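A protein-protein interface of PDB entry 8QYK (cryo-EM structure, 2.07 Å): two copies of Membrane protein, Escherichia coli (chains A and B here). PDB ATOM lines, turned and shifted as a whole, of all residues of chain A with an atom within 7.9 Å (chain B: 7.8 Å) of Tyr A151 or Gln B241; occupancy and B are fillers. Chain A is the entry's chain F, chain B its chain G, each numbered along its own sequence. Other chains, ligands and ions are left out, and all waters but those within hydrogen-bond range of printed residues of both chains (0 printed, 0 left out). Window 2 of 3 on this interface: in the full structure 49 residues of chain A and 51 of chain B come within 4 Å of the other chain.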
ATOM      1  N   ALA A 100       0.185 -18.968 -14.301  1.00  0.00           N
ATOM      2  CA  ALA A 100      -0.466 -19.129 -13.011  1.00  0.00           C
ATOM      3  C   ALA A 100      -1.876 -19.678 -13.195  1.00  0.00           C
ATOM      4  O   ALA A 100      -2.355 -19.880 -14.312  1.00  0.00           O
ATOM      5  CB  ALA A 100      -0.501 -17.799 -12.254  1.00  0.00           C
ATOM      6  N   HIS A 101      -2.539 -19.925 -12.068  1.00  0.00           N
ATOM      7  CA  HIS A 101      -3.911 -20.409 -12.101  1.00  0.00           C
ATOM      8  C   HIS A 101      -4.825 -19.367 -12.734  1.00  0.00           C
ATOM      9  O   HIS A 101      -4.734 -18.174 -12.431  1.00  0.00           O
ATOM     10  CB  HIS A 101      -4.390 -20.746 -10.689  1.00  0.00           C
ATOM     11  CG  HIS A 101      -5.850 -21.065 -10.605  1.00  0.00           C
ATOM     12  ND1 HIS A 101      -6.804 -20.114 -10.308  1.00  0.00           N
ATOM     13  CD2 HIS A 101      -6.520 -22.229 -10.774  1.00  0.00           C
ATOM     14  CE1 HIS A 101      -7.998 -20.679 -10.301  1.00  0.00           C
ATOM     15  NE2 HIS A 101      -7.854 -21.962 -10.581  1.00  0.00           N
ATOM     16  N   ASN A 102      -5.707 -19.831 -13.621  1.00  0.00           N
ATOM     17  CA  ASN A 102      -6.672 -18.972 -14.310  1.00  0.00           C
ATOM     18  C   ASN A 102      -5.974 -17.859 -15.092  1.00  0.00           C
ATOM     19  O   ASN A 102      -6.432 -16.714 -15.123  1.00  0.00           O
ATOM     20  CB  ASN A 102      -7.691 -18.391 -13.326  1.00  0.00           C
ATOM     21  CG  ASN A 102      -9.063 -18.213 -13.942  1.00  0.00           C
ATOM     22  OD1 ASN A 102      -9.206 -18.168 -15.164  1.00  0.00           O
ATOM     23  ND2 ASN A 102     -10.081 -18.114 -13.096  1.00  0.00           N
ATOM     24  N   GLN A 103      -4.856 -18.198 -15.730  1.00  0.00           N
ATOM     25  CA  GLN A 103      -4.102 -17.268 -16.559  1.00  0.00           C
ATOM     26  C   GLN A 103      -3.933 -17.858 -17.952  1.00  0.00           C
ATOM     27  O   GLN A 103      -3.746 -19.069 -18.104  1.00  0.00           O
ATOM     28  CB  GLN A 103      -2.731 -16.960 -15.945  1.00  0.00           C
ATOM     29  CG  GLN A 103      -1.970 -15.847 -16.650  1.00  0.00           C
ATOM     30  CD  GLN A 103      -0.543 -15.711 -16.158  1.00  0.00           C
ATOM     31  OE1 GLN A 103      -0.183 -16.240 -15.107  1.00  0.00           O
ATOM     32  NE2 GLN A 103       0.280 -15.001 -16.920  1.00  0.00           N
ATOM     33  N   THR A 143      -0.109 -28.674 -19.000  1.00  0.00           N
ATOM     34  CA  THR A 143      -0.801 -28.286 -17.780  1.00  0.00           C
ATOM     35  C   THR A 143      -0.708 -29.436 -16.785  1.00  0.00           C
ATOM     36  O   THR A 143      -0.506 -30.590 -17.170  1.00  0.00           O
ATOM     37  CB  THR A 143      -2.271 -27.926 -18.062  1.00  0.00           C
ATOM     38  OG1 THR A 143      -2.341 -27.053 -19.196  1.00  0.00           O
ATOM     39  CG2 THR A 143      -2.900 -27.213 -16.872  1.00  0.00           C
ATOM     40  N   ASP A 146      -3.639 -32.141 -12.014  1.00  0.00           N
ATOM     41  CA  ASP A 146      -4.583 -31.860 -10.947  1.00  0.00           C
ATOM     42  C   ASP A 146      -5.694 -30.937 -11.444  1.00  0.00           C
ATOM     43  O   ASP A 146      -5.652 -30.408 -12.556  1.00  0.00           O
ATOM     44  CB  ASP A 146      -3.868 -31.236  -9.748  1.00  0.00           C
ATOM     45  CG  ASP A 146      -3.349 -32.275  -8.774  1.00  0.00           C
ATOM     46  OD1 ASP A 146      -4.131 -33.165  -8.377  1.00  0.00           O
ATOM     47  OD2 ASP A 146      -2.159 -32.200  -8.402  1.00  0.00           O
ATOM     48  N   GLY A 147      -6.702 -30.749 -10.596  1.00  0.00           N
ATOM     49  CA  GLY A 147      -7.832 -29.912 -10.942  1.00  0.00           C
ATOM     50  C   GLY A 147      -8.748 -30.575 -11.951  1.00  0.00           C
ATOM     51  O   GLY A 147      -8.604 -31.746 -12.309  1.00  0.00           O
ATOM     52  N   SER A 148      -9.719 -29.795 -12.420  1.00  0.00           N
ATOM     53  CA  SER A 148     -10.654 -30.292 -13.420  1.00  0.00           C
ATOM     54  C   SER A 148      -9.942 -30.481 -14.753  1.00  0.00           C
ATOM     55  O   SER A 148      -9.237 -29.586 -15.228  1.00  0.00           O
ATOM     56  CB  SER A 148     -11.830 -29.331 -13.573  1.00  0.00           C
ATOM     57  OG  SER A 148     -12.717 -29.769 -14.589  1.00  0.00           O
ATOM     58  N   TYR A 149     -10.126 -31.659 -15.354  1.00  0.00           N
ATOM     59  CA  TYR A 149      -9.459 -31.964 -16.616  1.00  0.00           C
ATOM     60  C   TYR A 149      -9.963 -31.060 -17.735  1.00  0.00           C
ATOM     61  O   TYR A 149      -9.172 -30.532 -18.528  1.00  0.00           O
ATOM     62  CB  TYR A 149      -9.669 -33.440 -16.957  1.00  0.00           C
ATOM     63  CG  TYR A 149      -8.970 -33.915 -18.209  1.00  0.00           C
ATOM     64  CD1 TYR A 149      -7.584 -33.990 -18.266  1.00  0.00           C
ATOM     65  CD2 TYR A 149      -9.693 -34.317 -19.323  1.00  0.00           C
ATOM     66  CE1 TYR A 149      -6.939 -34.433 -19.403  1.00  0.00           C
ATOM     67  CE2 TYR A 149      -9.058 -34.762 -20.464  1.00  0.00           C
ATOM     68  CZ  TYR A 149      -7.682 -34.818 -20.499  1.00  0.00           C
ATOM     69  OH  TYR A 149      -7.046 -35.262 -21.635  1.00  0.00           O
ATOM     70  N   LEU A 150     -11.282 -30.857 -17.803  1.00  0.00           N
ATOM     71  CA  LEU A 150     -11.846 -29.959 -18.804  1.00  0.00           C
ATOM     72  C   LEU A 150     -11.381 -28.523 -18.587  1.00  0.00           C
ATOM     73  O   LEU A 150     -11.123 -27.797 -19.553  1.00  0.00           O
ATOM     74  CB  LEU A 150     -13.374 -30.037 -18.783  1.00  0.00           C
ATOM     75  CG  LEU A 150     -14.067 -31.131 -19.606  1.00  0.00           C
ATOM     76  CD1 LEU A 150     -13.756 -30.967 -21.086  1.00  0.00           C
ATOM     77  CD2 LEU A 150     -13.709 -32.534 -19.127  1.00  0.00           C
ATOM     78  N   TYR A 151     -11.281 -28.094 -17.326  1.00  0.00           N
ATOM     79  CA  TYR A 151     -10.806 -26.743 -17.032  1.00  0.00           C
ATOM     80  C   TYR A 151      -9.381 -26.546 -17.532  1.00  0.00           C
ATOM     81  O   TYR A 151      -9.061 -25.524 -18.151  1.00  0.00           O
ATOM     82  CB  TYR A 151     -10.896 -26.480 -15.528  1.00  0.00           C
ATOM     83  CG  TYR A 151     -10.311 -25.161 -15.070  1.00  0.00           C
ATOM     84  CD1 TYR A 151     -10.479 -24.001 -15.816  1.00  0.00           C
ATOM     85  CD2 TYR A 151      -9.601 -25.075 -13.878  1.00  0.00           C
ATOM     86  CE1 TYR A 151      -9.947 -22.798 -15.396  1.00  0.00           C
ATOM     87  CE2 TYR A 151      -9.067 -23.876 -13.449  1.00  0.00           C
ATOM     88  CZ  TYR A 151      -9.243 -22.741 -14.210  1.00  0.00           C
ATOM     89  OH  TYR A 151      -8.712 -21.545 -13.783  1.00  0.00           O
ATOM     90  N   ASN A 152      -8.510 -27.523 -17.276  1.00  0.00           N
ATOM     91  CA  ASN A 152      -7.129 -27.426 -17.732  1.00  0.00           C
ATOM     92  C   ASN A 152      -7.046 -27.445 -19.253  1.00  0.00           C
ATOM     93  O   ASN A 152      -6.251 -26.705 -19.850  1.00  0.00           O
ATOM     94  CB  ASN A 152      -6.301 -28.560 -17.125  1.00  0.00           C
ATOM     95  CG  ASN A 152      -6.338 -28.560 -15.605  1.00  0.00           C
ATOM     96  OD1 ASN A 152      -6.058 -27.548 -14.962  1.00  0.00           O
ATOM     97  ND2 ASN A 152      -6.692 -29.700 -15.024  1.00  0.00           N
ATOM     98  N   LEU A 153      -7.857 -28.284 -19.903  1.00  0.00           N
ATOM     99  CA  LEU A 153      -7.871 -28.306 -21.362  1.00  0.00           C
ATOM    100  C   LEU A 153      -8.308 -26.960 -21.925  1.00  0.00           C
ATOM    101  O   LEU A 153      -7.700 -26.437 -22.867  1.00  0.00           O
ATOM    102  CB  LEU A 153      -8.797 -29.410 -21.866  1.00  0.00           C
ATOM    103  CG  LEU A 153      -8.886 -29.493 -23.392  1.00  0.00           C
ATOM    104  CD1 LEU A 153      -7.557 -29.910 -24.025  1.00  0.00           C
ATOM    105  CD2 LEU A 153     -10.035 -30.376 -23.841  1.00  0.00           C
ATOM    106  N   HIS A 154      -9.366 -26.378 -21.355  1.00  0.00           N
ATOM    107  CA  HIS A 154      -9.843 -25.087 -21.831  1.00  0.00           C
ATOM    108  C   HIS A 154      -8.802 -24.000 -21.603  1.00  0.00           C
ATOM    109  O   HIS A 154      -8.612 -23.126 -22.455  1.00  0.00           O
ATOM    110  CB  HIS A 154     -11.161 -24.728 -21.144  1.00  0.00           C
ATOM    111  CG  HIS A 154     -11.722 -23.405 -21.565  1.00  0.00           C
ATOM    112  ND1 HIS A 154     -12.087 -23.132 -22.865  1.00  0.00           N
ATOM    113  CD2 HIS A 154     -11.995 -22.285 -20.854  1.00  0.00           C
ATOM    114  CE1 HIS A 154     -12.554 -21.899 -22.939  1.00  0.00           C
ATOM    115  NE2 HIS A 154     -12.510 -21.364 -21.733  1.00  0.00           N
ATOM    116  N   LEU A 155      -8.111 -24.042 -20.462  1.00  0.00           N
ATOM    117  CA  LEU A 155      -7.083 -23.045 -20.178  1.00  0.00           C
ATOM    118  C   LEU A 155      -5.926 -23.150 -21.167  1.00  0.00           C
ATOM    119  O   LEU A 155      -5.464 -22.139 -21.708  1.00  0.00           O
ATOM    120  CB  LEU A 155      -6.589 -23.203 -18.737  1.00  0.00           C
ATOM    121  CG  LEU A 155      -5.760 -22.067 -18.132  1.00  0.00           C
ATOM    122  CD1 LEU A 155      -6.065 -21.919 -16.651  1.00  0.00           C
ATOM    123  CD2 LEU A 155      -4.275 -22.308 -18.340  1.00  0.00           C
ATOM    124  N   SER A 156      -5.447 -24.372 -21.420  1.00  0.00           N
ATOM    125  CA  SER A 156      -4.351 -24.552 -22.369  1.00  0.00           C
ATOM    126  C   SER A 156      -4.766 -24.141 -23.777  1.00  0.00           C
ATOM    127  O   SER A 156      -3.989 -23.508 -24.507  1.00  0.00           O
ATOM    128  CB  SER A 156      -3.877 -26.007 -22.355  1.00  0.00           C
ATOM    129  OG  SER A 156      -3.267 -26.338 -21.120  1.00  0.00           O
ATOM    130  N   LEU A 157      -5.990 -24.490 -24.176  1.00  0.00           N
ATOM    131  CA  LEU A 157      -6.479 -24.111 -25.495  1.00  0.00           C
ATOM    132  C   LEU A 157      -6.609 -22.596 -25.615  1.00  0.00           C
ATOM    133  O   LEU A 157      -6.312 -22.020 -26.670  1.00  0.00           O
ATOM    134  CB  LEU A 157      -7.813 -24.806 -25.755  1.00  0.00           C
ATOM    135  CG  LEU A 157      -8.244 -25.007 -27.204  1.00  0.00           C
ATOM    136  CD1 LEU A 157      -7.263 -25.917 -27.921  1.00  0.00           C
ATOM    137  CD2 LEU A 157      -9.647 -25.587 -27.261  1.00  0.00           C
ATOM    138  N   GLN A 158      -7.042 -21.935 -24.539  1.00  0.00           N
ATOM    139  CA  GLN A 158      -7.112 -20.478 -24.526  1.00  0.00           C
ATOM    140  C   GLN A 158      -5.725 -19.860 -24.647  1.00  0.00           C
ATOM    141  O   GLN A 158      -5.547 -18.852 -25.340  1.00  0.00           O
ATOM    142  CB  GLN A 158      -7.802 -20.007 -23.245  1.00  0.00           C
ATOM    143  CG  GLN A 158      -8.086 -18.520 -23.197  1.00  0.00           C
ATOM    144  CD  GLN A 158      -8.745 -18.096 -21.898  1.00  0.00           C
ATOM    145  OE1 GLN A 158      -9.142 -16.943 -21.737  1.00  0.00           O
ATOM    146  NE2 GLN A 158      -8.859 -19.031 -20.961  1.00  0.00           N
ATOM    147  N   PHE A 197      -0.208 -33.334 -20.945  1.00  0.00           N
ATOM    148  CA  PHE A 197      -0.291 -33.269 -19.489  1.00  0.00           C
ATOM    149  C   PHE A 197       0.899 -33.980 -18.860  1.00  0.00           C
ATOM    150  O   PHE A 197       0.768 -34.763 -17.917  1.00  0.00           O
ATOM    151  CB  PHE A 197      -1.607 -33.865 -18.996  1.00  0.00           C
ATOM    152  CG  PHE A 197      -2.822 -33.102 -19.442  1.00  0.00           C
ATOM    153  CD1 PHE A 197      -3.388 -33.340 -20.683  1.00  0.00           C
ATOM    154  CD2 PHE A 197      -3.396 -32.144 -18.621  1.00  0.00           C
ATOM    155  CE1 PHE A 197      -4.504 -32.636 -21.098  1.00  0.00           C
ATOM    156  CE2 PHE A 197      -4.511 -31.439 -19.030  1.00  0.00           C
ATOM    157  CZ  PHE A 197      -5.065 -31.684 -20.270  1.00  0.00           C
ATOM    158  N   ARG A 208       2.787 -25.987 -16.202  1.00  0.00           N
ATOM    159  CA  ARG A 208       1.902 -25.138 -16.999  1.00  0.00           C
ATOM    160  C   ARG A 208       2.767 -24.215 -17.849  1.00  0.00           C
ATOM    161  O   ARG A 208       3.014 -23.057 -17.503  1.00  0.00           O
ATOM    162  CB  ARG A 208       0.946 -24.356 -16.107  1.00  0.00           C
ATOM    163  CG  ARG A 208      -0.456 -24.231 -16.685  1.00  0.00           C
ATOM    164  CD  ARG A 208      -1.452 -23.680 -15.674  1.00  0.00           C
ATOM    165  NE  ARG A 208      -1.527 -24.491 -14.465  1.00  0.00           N
ATOM    166  CZ  ARG A 208      -1.090 -24.103 -13.275  1.00  0.00           C
ATOM    167  NH1 ARG A 208      -0.530 -22.918 -13.099  1.00  0.00           N
ATOM    168  NH2 ARG A 208      -1.217 -24.924 -12.237  1.00  0.00           N
ATOM    169  N   PHE B 104     -20.887 -24.975 -32.716  1.00  0.00           N
ATOM    170  CA  PHE B 104     -19.962 -26.035 -32.334  1.00  0.00           C
ATOM    171  C   PHE B 104     -20.666 -27.241 -31.726  1.00  0.00           C
ATOM    172  O   PHE B 104     -20.019 -28.039 -31.037  1.00  0.00           O
ATOM    173  CB  PHE B 104     -18.904 -25.493 -31.366  1.00  0.00           C
ATOM    174  CG  PHE B 104     -19.475 -24.866 -30.123  1.00  0.00           C
ATOM    175  CD1 PHE B 104     -19.786 -23.516 -30.093  1.00  0.00           C
ATOM    176  CD2 PHE B 104     -19.683 -25.622 -28.981  1.00  0.00           C
ATOM    177  CE1 PHE B 104     -20.306 -22.934 -28.953  1.00  0.00           C
ATOM    178  CE2 PHE B 104     -20.202 -25.045 -27.836  1.00  0.00           C
ATOM    179  CZ  PHE B 104     -20.512 -23.700 -27.822  1.00  0.00           C
ATOM    180  N   GLU B 161     -13.275 -28.605 -28.057  1.00  0.00           N
ATOM    181  CA  GLU B 161     -13.661 -28.542 -26.651  1.00  0.00           C
ATOM    182  C   GLU B 161     -15.034 -29.162 -26.432  1.00  0.00           C
ATOM    183  O   GLU B 161     -15.232 -29.910 -25.471  1.00  0.00           O
ATOM    184  CB  GLU B 161     -13.642 -27.093 -26.166  1.00  0.00           C
ATOM    185  CG  GLU B 161     -13.859 -26.931 -24.670  1.00  0.00           C
ATOM    186  CD  GLU B 161     -12.660 -27.375 -23.856  1.00  0.00           C
ATOM    187  OE1 GLU B 161     -11.532 -27.345 -24.392  1.00  0.00           O
ATOM    188  OE2 GLU B 161     -12.846 -27.753 -22.680  1.00  0.00           O
ATOM    189  N   CYS B 165     -15.953 -32.404 -24.281  1.00  0.00           N
ATOM    190  CA  CYS B 165     -17.012 -32.213 -23.299  1.00  0.00           C
ATOM    191  C   CYS B 165     -18.055 -33.315 -23.415  1.00  0.00           C
ATOM    192  O   CYS B 165     -18.392 -33.974 -22.428  1.00  0.00           O
ATOM    193  CB  CYS B 165     -17.656 -30.841 -23.493  1.00  0.00           C
ATOM    194  SG  CYS B 165     -16.815 -29.482 -22.658  1.00  0.00           S
ATOM    195  N   ASP B 169     -18.585 -35.299 -20.027  1.00  0.00           N
ATOM    196  CA  ASP B 169     -19.449 -34.406 -19.268  1.00  0.00           C
ATOM    197  C   ASP B 169     -20.398 -35.214 -18.392  1.00  0.00           C
ATOM    198  O   ASP B 169     -20.817 -36.317 -18.753  1.00  0.00           O
ATOM    199  CB  ASP B 169     -20.264 -33.487 -20.187  1.00  0.00           C
ATOM    200  CG  ASP B 169     -21.086 -32.472 -19.419  1.00  0.00           C
ATOM    201  OD1 ASP B 169     -20.650 -32.057 -18.325  1.00  0.00           O
ATOM    202  OD2 ASP B 169     -22.168 -32.086 -19.910  1.00  0.00           O
ATOM    203  N   GLU B 238     -16.967 -34.324 -13.952  1.00  0.00           N
ATOM    204  CA  GLU B 238     -16.534 -33.228 -14.806  1.00  0.00           C
ATOM    205  C   GLU B 238     -17.732 -32.446 -15.329  1.00  0.00           C
ATOM    206  O   GLU B 238     -18.784 -33.008 -15.645  1.00  0.00           O
ATOM    207  CB  GLU B 238     -15.703 -33.756 -15.975  1.00  0.00           C
ATOM    208  CG  GLU B 238     -14.393 -34.407 -15.563  1.00  0.00           C
ATOM    209  CD  GLU B 238     -13.392 -33.406 -15.019  1.00  0.00           C
ATOM    210  OE1 GLU B 238     -13.386 -32.250 -15.494  1.00  0.00           O
ATOM    211  OE2 GLU B 238     -12.611 -33.774 -14.117  1.00  0.00           O
ATOM    212  N   VAL B 239     -17.564 -31.128 -15.414  1.00  0.00           N
ATOM    213  CA  VAL B 239     -18.595 -30.226 -15.914  1.00  0.00           C
ATOM    214  C   VAL B 239     -17.999 -29.410 -17.051  1.00  0.00           C
ATOM    215  O   VAL B 239     -16.945 -28.787 -16.887  1.00  0.00           O
ATOM    216  CB  VAL B 239     -19.133 -29.300 -14.806  1.00  0.00           C
ATOM    217  CG1 VAL B 239     -20.157 -28.328 -15.374  1.00  0.00           C
ATOM    218  CG2 VAL B 239     -19.734 -30.120 -13.676  1.00  0.00           C
ATOM    219  N   CYS B 240     -18.672 -29.416 -18.199  1.00  0.00           N
ATOM    220  CA  CYS B 240     -18.197 -28.652 -19.344  1.00  0.00           C
ATOM    221  C   CYS B 240     -18.325 -27.157 -19.081  1.00  0.00           C
ATOM    222  O   CYS B 240     -19.297 -26.694 -18.478  1.00  0.00           O
ATOM    223  CB  CYS B 240     -18.979 -29.027 -20.600  1.00  0.00           C
ATOM    224  SG  CYS B 240     -18.336 -28.260 -22.102  1.00  0.00           S
ATOM    225  N   GLN B 241     -17.332 -26.399 -19.544  1.00  0.00           N
ATOM    226  CA  GLN B 241     -17.299 -24.956 -19.353  1.00  0.00           C
ATOM    227  C   GLN B 241     -17.772 -24.179 -20.573  1.00  0.00           C
ATOM    228  O   GLN B 241     -17.819 -22.945 -20.523  1.00  0.00           O
ATOM    229  CB  GLN B 241     -15.884 -24.509 -18.972  1.00  0.00           C
ATOM    230  CG  GLN B 241     -15.452 -24.970 -17.594  1.00  0.00           C
ATOM    231  CD  GLN B 241     -14.059 -24.503 -17.230  1.00  0.00           C
ATOM    232  OE1 GLN B 241     -13.347 -23.932 -18.057  1.00  0.00           O
ATOM    233  NE2 GLN B 241     -13.665 -24.736 -15.985  1.00  0.00           N
ATOM    234  N   LEU B 242     -18.123 -24.858 -21.661  1.00  0.00           N
ATOM    235  CA  LEU B 242     -18.660 -24.167 -22.820  1.00  0.00           C
ATOM    236  C   LEU B 242     -20.105 -23.746 -22.568  1.00  0.00           C
ATOM    237  O   LEU B 242     -20.828 -24.350 -21.770  1.00  0.00           O
ATOM    238  CB  LEU B 242     -18.575 -25.046 -24.067  1.00  0.00           C
ATOM    239  CG  LEU B 242     -17.193 -25.151 -24.714  1.00  0.00           C
ATOM    240  CD1 LEU B 242     -17.247 -26.023 -25.955  1.00  0.00           C
ATOM    241  CD2 LEU B 242     -16.648 -23.771 -25.047  1.00  0.00           C
ATOM    242  N   VAL B 243     -20.522 -22.693 -23.267  1.00  0.00           N
ATOM    243  CA  VAL B 243     -21.862 -22.132 -23.111  1.00  0.00           C
ATOM    244  C   VAL B 243     -22.825 -22.982 -23.940  1.00  0.00           C
ATOM    245  O   VAL B 243     -22.948 -22.814 -25.154  1.00  0.00           O
ATOM    246  CB  VAL B 243     -21.912 -20.652 -23.501  1.00  0.00           C
ATOM    247  CG1 VAL B 243     -21.243 -19.814 -22.429  1.00  0.00           C
ATOM    248  CG2 VAL B 243     -21.199 -20.415 -24.829  1.00  0.00           C
ATOM    249  N   MET B 244     -23.503 -23.919 -23.277  1.00  0.00           N
ATOM    250  CA  MET B 244     -24.500 -24.735 -23.968  1.00  0.00           C
ATOM    251  C   MET B 244     -25.671 -23.916 -24.499  1.00  0.00           C
ATOM    252  O   MET B 244     -26.007 -24.065 -25.687  1.00  0.00           O
ATOM    253  CB  MET B 244     -24.973 -25.863 -23.044  1.00  0.00           C
ATOM    254  CG  MET B 244     -23.907 -26.902 -22.730  1.00  0.00           C
ATOM    255  SD  MET B 244     -24.508 -28.201 -21.634  1.00  0.00           S
ATOM    256  CE  MET B 244     -23.019 -29.167 -21.399  1.00  0.00           C
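A ring nitrogen (NE2) of His A101 lies within hydrogen-bond range of the side-chain hydroxyl (OH) of Tyr A151, at 3.3 Å.
N of Asn A102 lies close to OH of Tyr A151, at 3.5 Å.
The backbone carbonyl oxygen (O) of Ser A148 lies within hydrogen-bond range of the side-chain amide nitrogen (ND2) of Asn A152, 2.6 Å away.
The side-chain sulfur (SG) of Cys B165 forms a disulfide with the side-chain sulfur (SG) of Cys B240 (2.0 Å).
OE1 of Glu B238 sits at hydrogen-bond distance from OG of Ser A148 (2.7 Å).
N of Tyr A149 sits at hydrogen-bond distance from OE1 of Glu B238, 3.3 Å away.
The backbone NH of Leu A150 is in hydrogen-bond range of the side-chain carboxylate of Glu B238.
Glu B161 touches Leu A150 (OE2 to O, 3.6 Å).
Leu A150 touches Cys B165.
Tyr A151 touches Gln B241 (CD1 to NE2, 3.3 Å).
OE1 of Glu B161 touches CD2 of Leu A153, at 3.4 Å.
Glu B161 touches His A154.
His A154 touches Gln B241.
Leu A157 touches Glu B161.
No position is printed for both chains.
Of the 10 pairs that touch across the chains among the printed residues, none has its exchanged pair printed and touching as well.
Tyr A151 touches just one residue of chain B: Gln B241.
Gln B241 touches two residues of chain A.
No residue of chain A comes within 4 Å of Cys B240.
Of the printed residues of chain B, Tyr A149 touches Glu B238 (3.3 Å).
Printed residues of chain A within 4 Å of Glu B238: Ser A148, Tyr A149 and Leu A150.
Of the printed residues of chain B, Ser A148 touches Glu B238 (2.7 Å).
Met B244 touches none of the printed residues of chain A.
The nearest residue of chain A that does not touch Gln B241 is Leu A150 (4.7 Å).
Along chain B the printed residues that touch a printed residue of chain A span positions 161 to 241.
Among the printed residues, 10 pairs touch across the chains.
Among the printed residues, no Asp or Glu carboxylate lies within 4 Å of a Lys or Arg side-chain nitrogen of the other chain.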
